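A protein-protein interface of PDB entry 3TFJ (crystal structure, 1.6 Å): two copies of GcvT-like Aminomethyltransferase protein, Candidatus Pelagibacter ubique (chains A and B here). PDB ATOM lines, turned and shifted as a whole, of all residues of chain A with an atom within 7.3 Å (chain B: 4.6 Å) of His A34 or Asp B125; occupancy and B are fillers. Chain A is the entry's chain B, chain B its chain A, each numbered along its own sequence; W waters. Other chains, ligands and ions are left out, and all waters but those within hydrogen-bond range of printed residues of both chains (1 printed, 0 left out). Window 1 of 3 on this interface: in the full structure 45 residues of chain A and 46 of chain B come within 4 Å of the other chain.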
ATOM      1  N   SER A   9      -7.119  34.551   2.753  1.00  0.00           N
ATOM      2  CA  SER A   9      -7.937  33.736   3.645  1.00  0.00           C
ATOM      3  C   SER A   9      -7.833  32.287   3.158  1.00  0.00           C
ATOM      4  O   SER A   9      -7.397  32.045   2.011  1.00  0.00           O
ATOM      5  CB  SER A   9      -9.428  34.165   3.602  1.00  0.00           C
ATOM      6  OG  SER A   9      -9.941  34.015   2.273  1.00  0.00           O
ATOM      7  N   ARG A  10      -8.297  31.323   3.943  1.00  0.00           N
ATOM      8  CA  ARG A  10      -8.364  29.942   3.469  1.00  0.00           C
ATOM      9  C   ARG A  10      -9.089  29.790   2.123  1.00  0.00           C
ATOM     10  O   ARG A  10      -8.687  29.002   1.252  1.00  0.00           O
ATOM     11  CB  ARG A  10      -8.935  28.998   4.537  1.00  0.00           C
ATOM     12  CG  ARG A  10      -9.037  27.548   4.134  1.00  0.00           C
ATOM     13  CD  ARG A  10      -9.566  26.697   5.290  1.00  0.00           C
ATOM     14  NE  ARG A  10      -9.485  25.290   4.961  1.00  0.00           N
ATOM     15  CZ  ARG A  10     -10.372  24.574   4.268  1.00  0.00           C
ATOM     16  NH1 ARG A  10     -11.568  25.055   3.965  1.00  0.00           N
ATOM     17  NH2 ARG A  10     -10.117  23.290   3.983  1.00  0.00           N
ATOM     18  N   ARG A  11     -10.173  30.554   1.963  1.00  0.00           N
ATOM     19  CA  ARG A  11     -11.025  30.448   0.780  1.00  0.00           C
ATOM     20  C   ARG A  11     -10.283  30.878  -0.492  1.00  0.00           C
ATOM     21  O   ARG A  11     -10.588  30.377  -1.573  1.00  0.00           O
ATOM     22  CB  ARG A  11     -12.250  31.331   0.990  1.00  0.00           C
ATOM     23  CG  ARG A  11     -13.234  31.335  -0.087  1.00  0.00           C
ATOM     24  CD  ARG A  11     -14.531  32.106   0.307  1.00  0.00           C
ATOM     25  NE  ARG A  11     -14.227  33.505   0.539  1.00  0.00           N
ATOM     26  CZ  ARG A  11     -13.943  34.414  -0.358  1.00  0.00           C
ATOM     27  NH1 ARG A  11     -13.955  34.088  -1.608  1.00  0.00           N
ATOM     28  NH2 ARG A  11     -13.612  35.637   0.037  1.00  0.00           N
ATOM     29  N   LEU A  12      -9.370  31.847  -0.374  1.00  0.00           N
ATOM     30  CA  LEU A  12      -8.474  32.219  -1.499  1.00  0.00           C
ATOM     31  C   LEU A  12      -7.265  31.296  -1.426  1.00  0.00           C
ATOM     32  O   LEU A  12      -6.266  31.572  -0.817  1.00  0.00           O
ATOM     33  CB  LEU A  12      -8.065  33.668  -1.437  1.00  0.00           C
ATOM     34  CG  LEU A  12      -9.143  34.727  -1.612  1.00  0.00           C
ATOM     35  CD1 LEU A  12      -8.566  36.146  -1.803  1.00  0.00           C
ATOM     36  CD2 LEU A  12     -10.175  34.344  -2.571  1.00  0.00           C
ATOM     37  N   ARG A  13      -7.435  30.127  -2.004  1.00  0.00           N
ATOM     38  CA  ARG A  13      -6.523  29.063  -1.729  1.00  0.00           C
ATOM     39  C   ARG A  13      -5.083  29.350  -2.141  1.00  0.00           C
ATOM     40  O   ARG A  13      -4.825  29.830  -3.229  1.00  0.00           O
ATOM     41  CB  ARG A  13      -6.986  27.788  -2.359  1.00  0.00           C
ATOM     42  CG  ARG A  13      -8.317  27.224  -1.872  1.00  0.00           C
ATOM     43  CD  ARG A  13      -8.777  25.973  -2.607  1.00  0.00           C
ATOM     44  NE  ARG A  13      -9.173  26.281  -3.960  1.00  0.00           N
ATOM     45  CZ  ARG A  13      -9.489  25.353  -4.865  1.00  0.00           C
ATOM     46  NH1 ARG A  13      -9.455  24.068  -4.559  1.00  0.00           N
ATOM     47  NH2 ARG A  13      -9.819  25.754  -6.099  1.00  0.00           N
ATOM     48  N   SER A  14      -4.172  28.959  -1.282  1.00  0.00           N
ATOM     49  CA  SER A  14      -2.741  28.966  -1.616  1.00  0.00           C
ATOM     50  C   SER A  14      -2.383  27.698  -2.362  1.00  0.00           C
ATOM     51  O   SER A  14      -3.236  26.839  -2.594  1.00  0.00           O
ATOM     52  CB  SER A  14      -1.905  29.093  -0.371  1.00  0.00           C
ATOM     53  OG  SER A  14      -2.088  27.998   0.475  1.00  0.00           O
ATOM     54  N   ILE A  31      -7.242  36.105  -8.632  1.00  0.00           N
ATOM     55  CA  ILE A  31      -7.919  34.926  -8.091  1.00  0.00           C
ATOM     56  C   ILE A  31      -8.550  34.216  -9.290  1.00  0.00           C
ATOM     57  O   ILE A  31      -9.220  34.838 -10.136  1.00  0.00           O
ATOM     58  CB  ILE A  31      -8.978  35.231  -7.040  1.00  0.00           C
ATOM     59  CG1 ILE A  31      -8.329  35.838  -5.817  1.00  0.00           C
ATOM     60  CG2 ILE A  31      -9.868  33.984  -6.625  1.00  0.00           C
ATOM     61  CD1 ILE A  31      -7.283  34.961  -5.121  1.00  0.00           C
ATOM     62  N   TYR A  32      -8.305  32.907  -9.347  1.00  0.00           N
ATOM     63  CA  TYR A  32      -8.697  32.105 -10.501  1.00  0.00           C
ATOM     64  C   TYR A  32      -9.105  30.757  -9.940  1.00  0.00           C
ATOM     65  O   TYR A  32      -8.313  30.149  -9.199  1.00  0.00           O
ATOM     66  CB  TYR A  32      -7.512  32.016 -11.424  1.00  0.00           C
ATOM     67  CG  TYR A  32      -7.713  31.546 -12.839  1.00  0.00           C
ATOM     68  CD1 TYR A  32      -7.718  32.427 -13.891  1.00  0.00           C
ATOM     69  CD2 TYR A  32      -7.794  30.191 -13.147  1.00  0.00           C
ATOM     70  CE1 TYR A  32      -7.818  31.952 -15.204  1.00  0.00           C
ATOM     71  CE2 TYR A  32      -7.862  29.755 -14.399  1.00  0.00           C
ATOM     72  CZ  TYR A  32      -7.902  30.630 -15.454  1.00  0.00           C
ATOM     73  OH  TYR A  32      -7.915  30.089 -16.721  1.00  0.00           O
ATOM     74  N   ASN A  33     -10.354  30.304 -10.188  1.00  0.00           N
ATOM     75  CA  ASN A  33     -10.835  29.093  -9.529  1.00  0.00           C
ATOM     76  C   ASN A  33     -10.572  29.104  -8.006  1.00  0.00           C
ATOM     77  O   ASN A  33     -10.140  28.127  -7.431  1.00  0.00           O
ATOM     78  CB  ASN A  33     -10.240  27.838 -10.166  1.00  0.00           C
ATOM     79  CG  ASN A  33     -10.799  27.605 -11.564  1.00  0.00           C
ATOM     80  OD1 ASN A  33     -12.006  27.674 -11.752  1.00  0.00           O
ATOM     81  ND2 ASN A  33      -9.934  27.309 -12.542  1.00  0.00           N
ATOM     82  N   HIS A  34     -10.945  30.194  -7.373  1.00  0.00           N
ATOM     83  CA  HIS A  34     -10.869  30.265  -5.914  1.00  0.00           C
ATOM     84  C   HIS A  34      -9.452  29.918  -5.381  1.00  0.00           C
ATOM     85  O   HIS A  34      -9.280  29.307  -4.354  1.00  0.00           O
ATOM     86  CB  HIS A  34     -11.907  29.297  -5.260  1.00  0.00           C
ATOM     87  CG  HIS A  34     -13.259  29.389  -5.834  1.00  0.00           C
ATOM     88  ND1 HIS A  34     -13.794  28.520  -6.752  1.00  0.00           N
ATOM     89  CD2 HIS A  34     -14.193  30.322  -5.628  1.00  0.00           C
ATOM     90  CE1 HIS A  34     -15.035  28.910  -7.056  1.00  0.00           C
ATOM     91  NE2 HIS A  34     -15.299  29.988  -6.364  1.00  0.00           N
ATOM     92  N   MET A  35      -8.459  30.395  -6.105  1.00  0.00           N
ATOM     93  CA  MET A  35      -7.070  30.121  -5.845  1.00  0.00           C
ATOM     94  C   MET A  35      -6.199  31.308  -6.299  1.00  0.00           C
ATOM     95  O   MET A  35      -6.477  31.974  -7.305  1.00  0.00           O
ATOM     96  CB  MET A  35      -6.645  28.812  -6.482  1.00  0.00           C
ATOM     97  CG  MET A  35      -5.228  28.380  -6.192  1.00  0.00           C
ATOM     98  SD  MET A  35      -4.915  26.640  -6.698  1.00  0.00           S
ATOM     99  CE  MET A  35      -5.876  25.745  -5.442  1.00  0.00           C
ATOM    100  N   LEU A  36      -5.132  31.532  -5.541  1.00  0.00           N
ATOM    101  CA  LEU A  36      -4.169  32.570  -5.840  1.00  0.00           C
ATOM    102  C   LEU A  36      -3.430  32.148  -7.135  1.00  0.00           C
ATOM    103  O   LEU A  36      -2.900  31.052  -7.245  1.00  0.00           O
ATOM    104  CB  LEU A  36      -3.156  32.727  -4.710  1.00  0.00           C
ATOM    105  CG  LEU A  36      -3.692  33.346  -3.385  1.00  0.00           C
ATOM    106  CD1 LEU A  36      -2.673  33.054  -2.278  1.00  0.00           C
ATOM    107  CD2 LEU A  36      -3.953  34.819  -3.572  1.00  0.00           C
ATOM    108  N   ALA A  62      -3.755  27.222 -10.104  1.00  0.00           N
ATOM    109  CA  ALA A  62      -5.155  27.646 -10.248  1.00  0.00           C
ATOM    110  C   ALA A  62      -5.849  27.101 -11.510  1.00  0.00           C
ATOM    111  O   ALA A  62      -7.109  27.171 -11.616  1.00  0.00           O
ATOM    112  CB  ALA A  62      -5.310  29.129 -10.173  1.00  0.00           C
ATOM    113  N   ARG A  64      -7.144  24.343 -12.307  1.00  0.00           N
ATOM    114  CA  ARG A  64      -7.578  23.171 -11.623  1.00  0.00           C
ATOM    115  C   ARG A  64      -7.952  22.066 -12.573  1.00  0.00           C
ATOM    116  O   ARG A  64      -8.264  22.337 -13.720  1.00  0.00           O
ATOM    117  CB  ARG A  64      -8.748  23.435 -10.725  1.00  0.00           C
ATOM    118  CG  ARG A  64      -8.621  24.603  -9.782  1.00  0.00           C
ATOM    119  CD  ARG A  64      -7.371  24.571  -8.920  1.00  0.00           C
ATOM    120  NE  ARG A  64      -7.354  23.422  -8.026  1.00  0.00           N
ATOM    121  CZ  ARG A  64      -6.290  22.819  -7.550  1.00  0.00           C
ATOM    122  NH1 ARG A  64      -5.081  23.162  -7.933  1.00  0.00           N
ATOM    123  NH2 ARG A  64      -6.466  21.791  -6.724  1.00  0.00           N
ATOM    124  N   ASP A 125     -11.568  29.846 -15.493  1.00  0.00           N
ATOM    125  CA  ASP A 125     -12.123  30.361 -14.237  1.00  0.00           C
ATOM    126  C   ASP A 125     -13.639  30.186 -14.122  1.00  0.00           C
ATOM    127  O   ASP A 125     -14.403  31.160 -14.093  1.00  0.00           O
ATOM    128  CB  ASP A 125     -11.664  31.801 -14.025  1.00  0.00           C
ATOM    129  CG  ASP A 125     -12.162  32.392 -12.731  1.00  0.00           C
ATOM    130  OD1 ASP A 125     -12.462  33.594 -12.718  1.00  0.00           O
ATOM    131  OD2 ASP A 125     -12.214  31.666 -11.740  1.00  0.00           O
ATOM    132  N   SER A 126     -14.081  28.936 -13.974  1.00  0.00           N
ATOM    133  CA  SER A 126     -15.447  28.688 -13.537  1.00  0.00           C
ATOM    134  C   SER A 126     -15.524  27.262 -12.966  1.00  0.00           C
ATOM    135  O   SER A 126     -14.695  26.401 -13.293  1.00  0.00           O
ATOM    136  CB  SER A 126     -16.494  28.840 -14.673  1.00  0.00           C
ATOM    137  OG  SER A 126     -16.371  27.796 -15.666  1.00  0.00           O
ATOM    138  N   ASP A 127     -16.561  26.984 -12.167  1.00  0.00           N
ATOM    139  CA  ASP A 127     -16.659  25.738 -11.420  1.00  0.00           C
ATOM    140  C   ASP A 127     -17.310  24.618 -12.224  1.00  0.00           C
ATOM    141  O   ASP A 127     -18.421  24.160 -11.892  1.00  0.00           O
ATOM    142  CB  ASP A 127     -17.365  25.935 -10.074  1.00  0.00           C
ATOM    143  CG  ASP A 127     -16.638  26.925  -9.148  1.00  0.00           C
ATOM    144  OD1 ASP A 127     -15.386  27.050  -9.232  1.00  0.00           O
ATOM    145  OD2 ASP A 127     -17.309  27.592  -8.322  1.00  0.00           O
ATOM    146  N   PHE A 130     -19.116  21.454 -10.787  1.00  0.00           N
ATOM    147  CA  PHE A 130     -20.500  21.413 -10.425  1.00  0.00           C
ATOM    148  C   PHE A 130     -21.408  21.213 -11.635  1.00  0.00           C
ATOM    149  O   PHE A 130     -22.471  20.595 -11.495  1.00  0.00           O
ATOM    150  CB  PHE A 130     -20.879  22.600  -9.557  1.00  0.00           C
ATOM    151  CG  PHE A 130     -20.121  22.623  -8.236  1.00  0.00           C
ATOM    152  CD1 PHE A 130     -20.133  21.539  -7.428  1.00  0.00           C
ATOM    153  CD2 PHE A 130     -19.375  23.731  -7.832  1.00  0.00           C
ATOM    154  CE1 PHE A 130     -19.453  21.531  -6.246  1.00  0.00           C
ATOM    155  CE2 PHE A 130     -18.701  23.716  -6.629  1.00  0.00           C
ATOM    156  CZ  PHE A 130     -18.663  22.588  -5.884  1.00  0.00           C
ATOM    157  N   GLU A 147     -12.166  16.825  -7.765  1.00  0.00           N
ATOM    158  CA  GLU A 147     -11.051  17.734  -8.048  1.00  0.00           C
ATOM    159  C   GLU A 147      -9.796  17.053  -7.450  1.00  0.00           C
ATOM    160  O   GLU A 147      -9.652  16.993  -6.208  1.00  0.00           O
ATOM    161  CB  GLU A 147     -11.329  19.122  -7.416  1.00  0.00           C
ATOM    162  CG  GLU A 147     -10.147  20.093  -7.677  1.00  0.00           C
ATOM    163  CD  GLU A 147     -10.459  21.524  -7.342  1.00  0.00           C
ATOM    164  OE1 GLU A 147      -9.601  22.194  -6.687  1.00  0.00           O
ATOM    165  OE2 GLU A 147     -11.568  21.984  -7.721  1.00  0.00           O
ATOM    166  N   ILE B  31     -11.965  38.408  -3.508  1.00  0.00           N
ATOM    167  CA  ILE B  31     -12.715  38.027  -4.722  1.00  0.00           C
ATOM    168  C   ILE B  31     -13.700  36.972  -4.296  1.00  0.00           C
ATOM    169  O   ILE B  31     -13.348  36.010  -3.600  1.00  0.00           O
ATOM    170  CB  ILE B  31     -11.803  37.491  -5.842  1.00  0.00           C
ATOM    171  CG1 ILE B  31     -10.837  38.587  -6.321  1.00  0.00           C
ATOM    172  CG2 ILE B  31     -12.621  36.911  -7.017  1.00  0.00           C
ATOM    173  CD1 ILE B  31     -11.527  39.830  -6.909  1.00  0.00           C
ATOM    174  N   TYR B  32     -14.956  37.166  -4.695  1.00  0.00           N
ATOM    175  CA  TYR B  32     -16.060  36.307  -4.256  1.00  0.00           C
ATOM    176  C   TYR B  32     -16.969  36.181  -5.484  1.00  0.00           C
ATOM    177  O   TYR B  32     -17.368  37.207  -6.030  1.00  0.00           O
ATOM    178  CB  TYR B  32     -16.703  36.989  -3.083  1.00  0.00           C
ATOM    179  CG  TYR B  32     -17.683  36.276  -2.244  1.00  0.00           C
ATOM    180  CD1 TYR B  32     -17.312  35.798  -1.019  1.00  0.00           C
ATOM    181  CD2 TYR B  32     -19.010  36.126  -2.610  1.00  0.00           C
ATOM    182  CE1 TYR B  32     -18.242  35.157  -0.182  1.00  0.00           C
ATOM    183  CE2 TYR B  32     -19.924  35.500  -1.784  1.00  0.00           C
ATOM    184  CZ  TYR B  32     -19.547  35.023  -0.587  1.00  0.00           C
ATOM    185  OH  TYR B  32     -20.498  34.478   0.284  1.00  0.00           O
ATOM    186  N   ASN B  33     -17.226  34.975  -5.944  1.00  0.00           N
ATOM    187  CA  ASN B  33     -17.991  34.793  -7.178  1.00  0.00           C
ATOM    188  C   ASN B  33     -17.456  35.635  -8.334  1.00  0.00           C
ATOM    189  O   ASN B  33     -18.201  36.331  -9.059  1.00  0.00           O
ATOM    190  CB  ASN B  33     -19.484  35.095  -6.926  1.00  0.00           C
ATOM    191  CG  ASN B  33     -20.155  34.026  -6.143  1.00  0.00           C
ATOM    192  OD1 ASN B  33     -19.978  32.828  -6.450  1.00  0.00           O
ATOM    193  ND2 ASN B  33     -20.936  34.416  -5.152  1.00  0.00           N
ATOM    194  N   ASN B 107     -22.630  25.032  -1.386  1.00  0.00           N
ATOM    195  CA  ASN B 107     -22.867  26.464  -1.188  1.00  0.00           C
ATOM    196  C   ASN B 107     -23.859  26.513  -0.042  1.00  0.00           C
ATOM    197  O   ASN B 107     -24.546  25.504   0.180  1.00  0.00           O
ATOM    198  CB  ASN B 107     -23.449  27.045  -2.485  1.00  0.00           C
ATOM    199  CG  ASN B 107     -23.356  28.564  -2.587  1.00  0.00           C
ATOM    200  OD1 ASN B 107     -24.158  29.311  -1.993  1.00  0.00           O
ATOM    201  ND2 ASN B 107     -22.365  29.047  -3.387  1.00  0.00           N
ATOM    202  N   ILE B 123     -26.118  33.594  -3.387  1.00  0.00           N
ATOM    203  CA  ILE B 123     -25.096  32.540  -3.190  1.00  0.00           C
ATOM    204  C   ILE B 123     -23.804  33.001  -2.476  1.00  0.00           C
ATOM    205  O   ILE B 123     -23.349  34.162  -2.575  1.00  0.00           O
ATOM    206  CB  ILE B 123     -24.736  31.886  -4.539  1.00  0.00           C
ATOM    207  CG1 ILE B 123     -24.231  32.885  -5.596  1.00  0.00           C
ATOM    208  CG2 ILE B 123     -25.952  31.060  -5.081  1.00  0.00           C
ATOM    209  CD1 ILE B 123     -23.406  32.269  -6.774  1.00  0.00           C
ATOM    210  N   ALA B 124     -23.204  32.035  -1.791  1.00  0.00           N
ATOM    211  CA  ALA B 124     -21.811  32.103  -1.303  1.00  0.00           C
ATOM    212  C   ALA B 124     -20.856  31.823  -2.487  1.00  0.00           C
ATOM    213  O   ALA B 124     -21.278  31.851  -3.654  1.00  0.00           O
ATOM    214  CB  ALA B 124     -21.624  31.097  -0.196  1.00  0.00           C
ATOM    215  N   ASP B 125     -19.573  31.675  -2.218  1.00  0.00           N
ATOM    216  CA  ASP B 125     -18.565  31.665  -3.288  1.00  0.00           C
ATOM    217  C   ASP B 125     -18.365  30.334  -4.048  1.00  0.00           C
ATOM    218  O   ASP B 125     -17.330  29.628  -3.871  1.00  0.00           O
ATOM    219  CB  ASP B 125     -17.243  32.108  -2.660  1.00  0.00           C
ATOM    220  CG  ASP B 125     -16.082  32.200  -3.664  1.00  0.00           C
ATOM    221  OD1 ASP B 125     -14.932  31.927  -3.224  1.00  0.00           O
ATOM    222  OD2 ASP B 125     -16.331  32.632  -4.846  1.00  0.00           O
ATOM    223  N   SER B 126     -19.363  29.971  -4.876  1.00  0.00           N
ATOM    224  CA  SER B 126     -19.208  28.876  -5.815  1.00  0.00           C
ATOM    225  C   SER B 126     -20.259  29.063  -6.892  1.00  0.00           C
ATOM    226  O   SER B 126     -21.291  29.732  -6.676  1.00  0.00           O
ATOM    227  CB  SER B 126     -19.349  27.507  -5.179  1.00  0.00           C
ATOM    228  OG  SER B 126     -20.686  27.203  -4.745  1.00  0.00           O
ATOM    229  N   TYR B 247     -18.578  29.523   3.226  1.00  0.00           N
ATOM    230  CA  TYR B 247     -18.231  28.453   2.279  1.00  0.00           C
ATOM    231  C   TYR B 247     -16.866  28.723   1.705  1.00  0.00           C
ATOM    232  O   TYR B 247     -16.563  29.843   1.248  1.00  0.00           O
ATOM    233  CB  TYR B 247     -19.229  28.296   1.124  1.00  0.00           C
ATOM    234  CG  TYR B 247     -18.830  27.220   0.163  1.00  0.00           C
ATOM    235  CD1 TYR B 247     -19.019  25.881   0.458  1.00  0.00           C
ATOM    236  CD2 TYR B 247     -18.143  27.538  -1.027  1.00  0.00           C
ATOM    237  CE1 TYR B 247     -18.576  24.895  -0.446  1.00  0.00           C
ATOM    238  CE2 TYR B 247     -17.703  26.546  -1.891  1.00  0.00           C
ATOM    239  CZ  TYR B 247     -17.917  25.255  -1.613  1.00  0.00           C
ATOM    240  OH  TYR B 247     -17.401  24.327  -2.526  1.00  0.00           O
HETATM  241  O   HOH W   1     -17.831  31.311  -7.595  1.00  0.00           O
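Ile B31 touches its own counterpart, Ile A31. Of the 9 pairs that touch across the chains among the printed residues, 1 has its exchanged pair printed and touching as well.
The guanidinium group (NH1) of Arg A11 lies within hydrogen-bond range of the backbone carbonyl oxygen (O) of Ile B31, at 2.8 Å. The guanidinium group (NH1) of Arg A11 is in salt-bridge range of the side-chain carboxylate (OD1) of Asp B125 (2.9 Å). The side-chain carboxylate (OD2) of Asp B125 lies within hydrogen-bond range of a ring nitrogen (NE2) of His A34 (3.2 Å).
The backbone NH (N) of Asn B33 lies within hydrogen-bond range of the side-chain carboxylate (OD2) of Asp B125, at 2.7 Å. OD1 of Asn B33 lies within hydrogen-bond range of N of Ser B126, at 3.3 Å. The side-chain amide nitrogen (ND2) of Asn B107 sits at hydrogen-bond distance from the side-chain hydroxyl (OG) of Ser B126 (2.8 Å). The side-chain hydroxyl (OG) of Ser A9 sits at hydrogen-bond distance from the backbone NH (N) of Leu A12 (3.5 Å). NE of Arg A13 lies within hydrogen-bond range of O of His A34 (3.1 Å). A ring nitrogen (ND1) of His A34 sits close to the side-chain carboxylate (OD1) of Asp A127.
Of chain B, only Asp B125 comes within 4 Å of His A34. Printed residues of chain A within 4 Å of Ile B31: Arg A11 (2.8 Å), Leu A12 (3.7 Å) and Ile A31 (3.8 Å). Ile B123 touches none of the printed residues of chain A. Of chain A, only Arg A11 (2.9 Å) and His A34 (3.0 Å) come within 4 Å of Asp B125. Of the printed residues of chain A, Ser B126 touches Asp A127. The nearest residue of chain B that does not touch His A34 is Ser B126 (4.1 Å). The nearest residue of chain A that does not touch Asp B125 is Asp A127 (4.9 Å). The nearest printed residue of chain A that does not touch Ser B126 is His A34 (4.1 Å).
Of the 19 printed residues of chain A, 6 touch a printed residue of chain B. Hydrophobic or aromatic side chains of chain A within 4 Å of the printed part of chain B: Leu A12, Ile A31, His A34 and Phe A130. Printed residues of chain B that touch a printed residue of chain A: Ile B31, Tyr B32, Asp B125, Ser B126 and Tyr B247. Hydrophobic or aromatic side chains of chain B that line the printed part of chain A: Ile B31, Tyr B32 and Tyr B247. Among the printed residues, Asp or Glu carboxylates within 4 Å of a Lys or Arg side-chain nitrogen of the other chain: Arg A11 with Asp B125.
Among the printed residues, pairs that only touch across the chains: Arg A11 with Tyr B32 (3.7 Å), Arg A11 with Tyr B247 (3.2 Å), Leu A12 with Ile B31 (3.7 Å), Ile A31 with Ile B31 (3.8 Å), Asp A127 with Ser B126 (3.4 Å) and Phe A130 with Tyr B247 (3.99 Å).
Water W1 lies within hydrogen-bond range of the side-chain amide oxygen (OD1) of Asn B33 (2.9 Å), a ring nitrogen (NE2) of His A34 (3.1 Å), the backbone NH (N) of Ser B126 (3.4 Å) and the side-chain carboxylate (OD2) of Asp B125 (3.4 Å).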
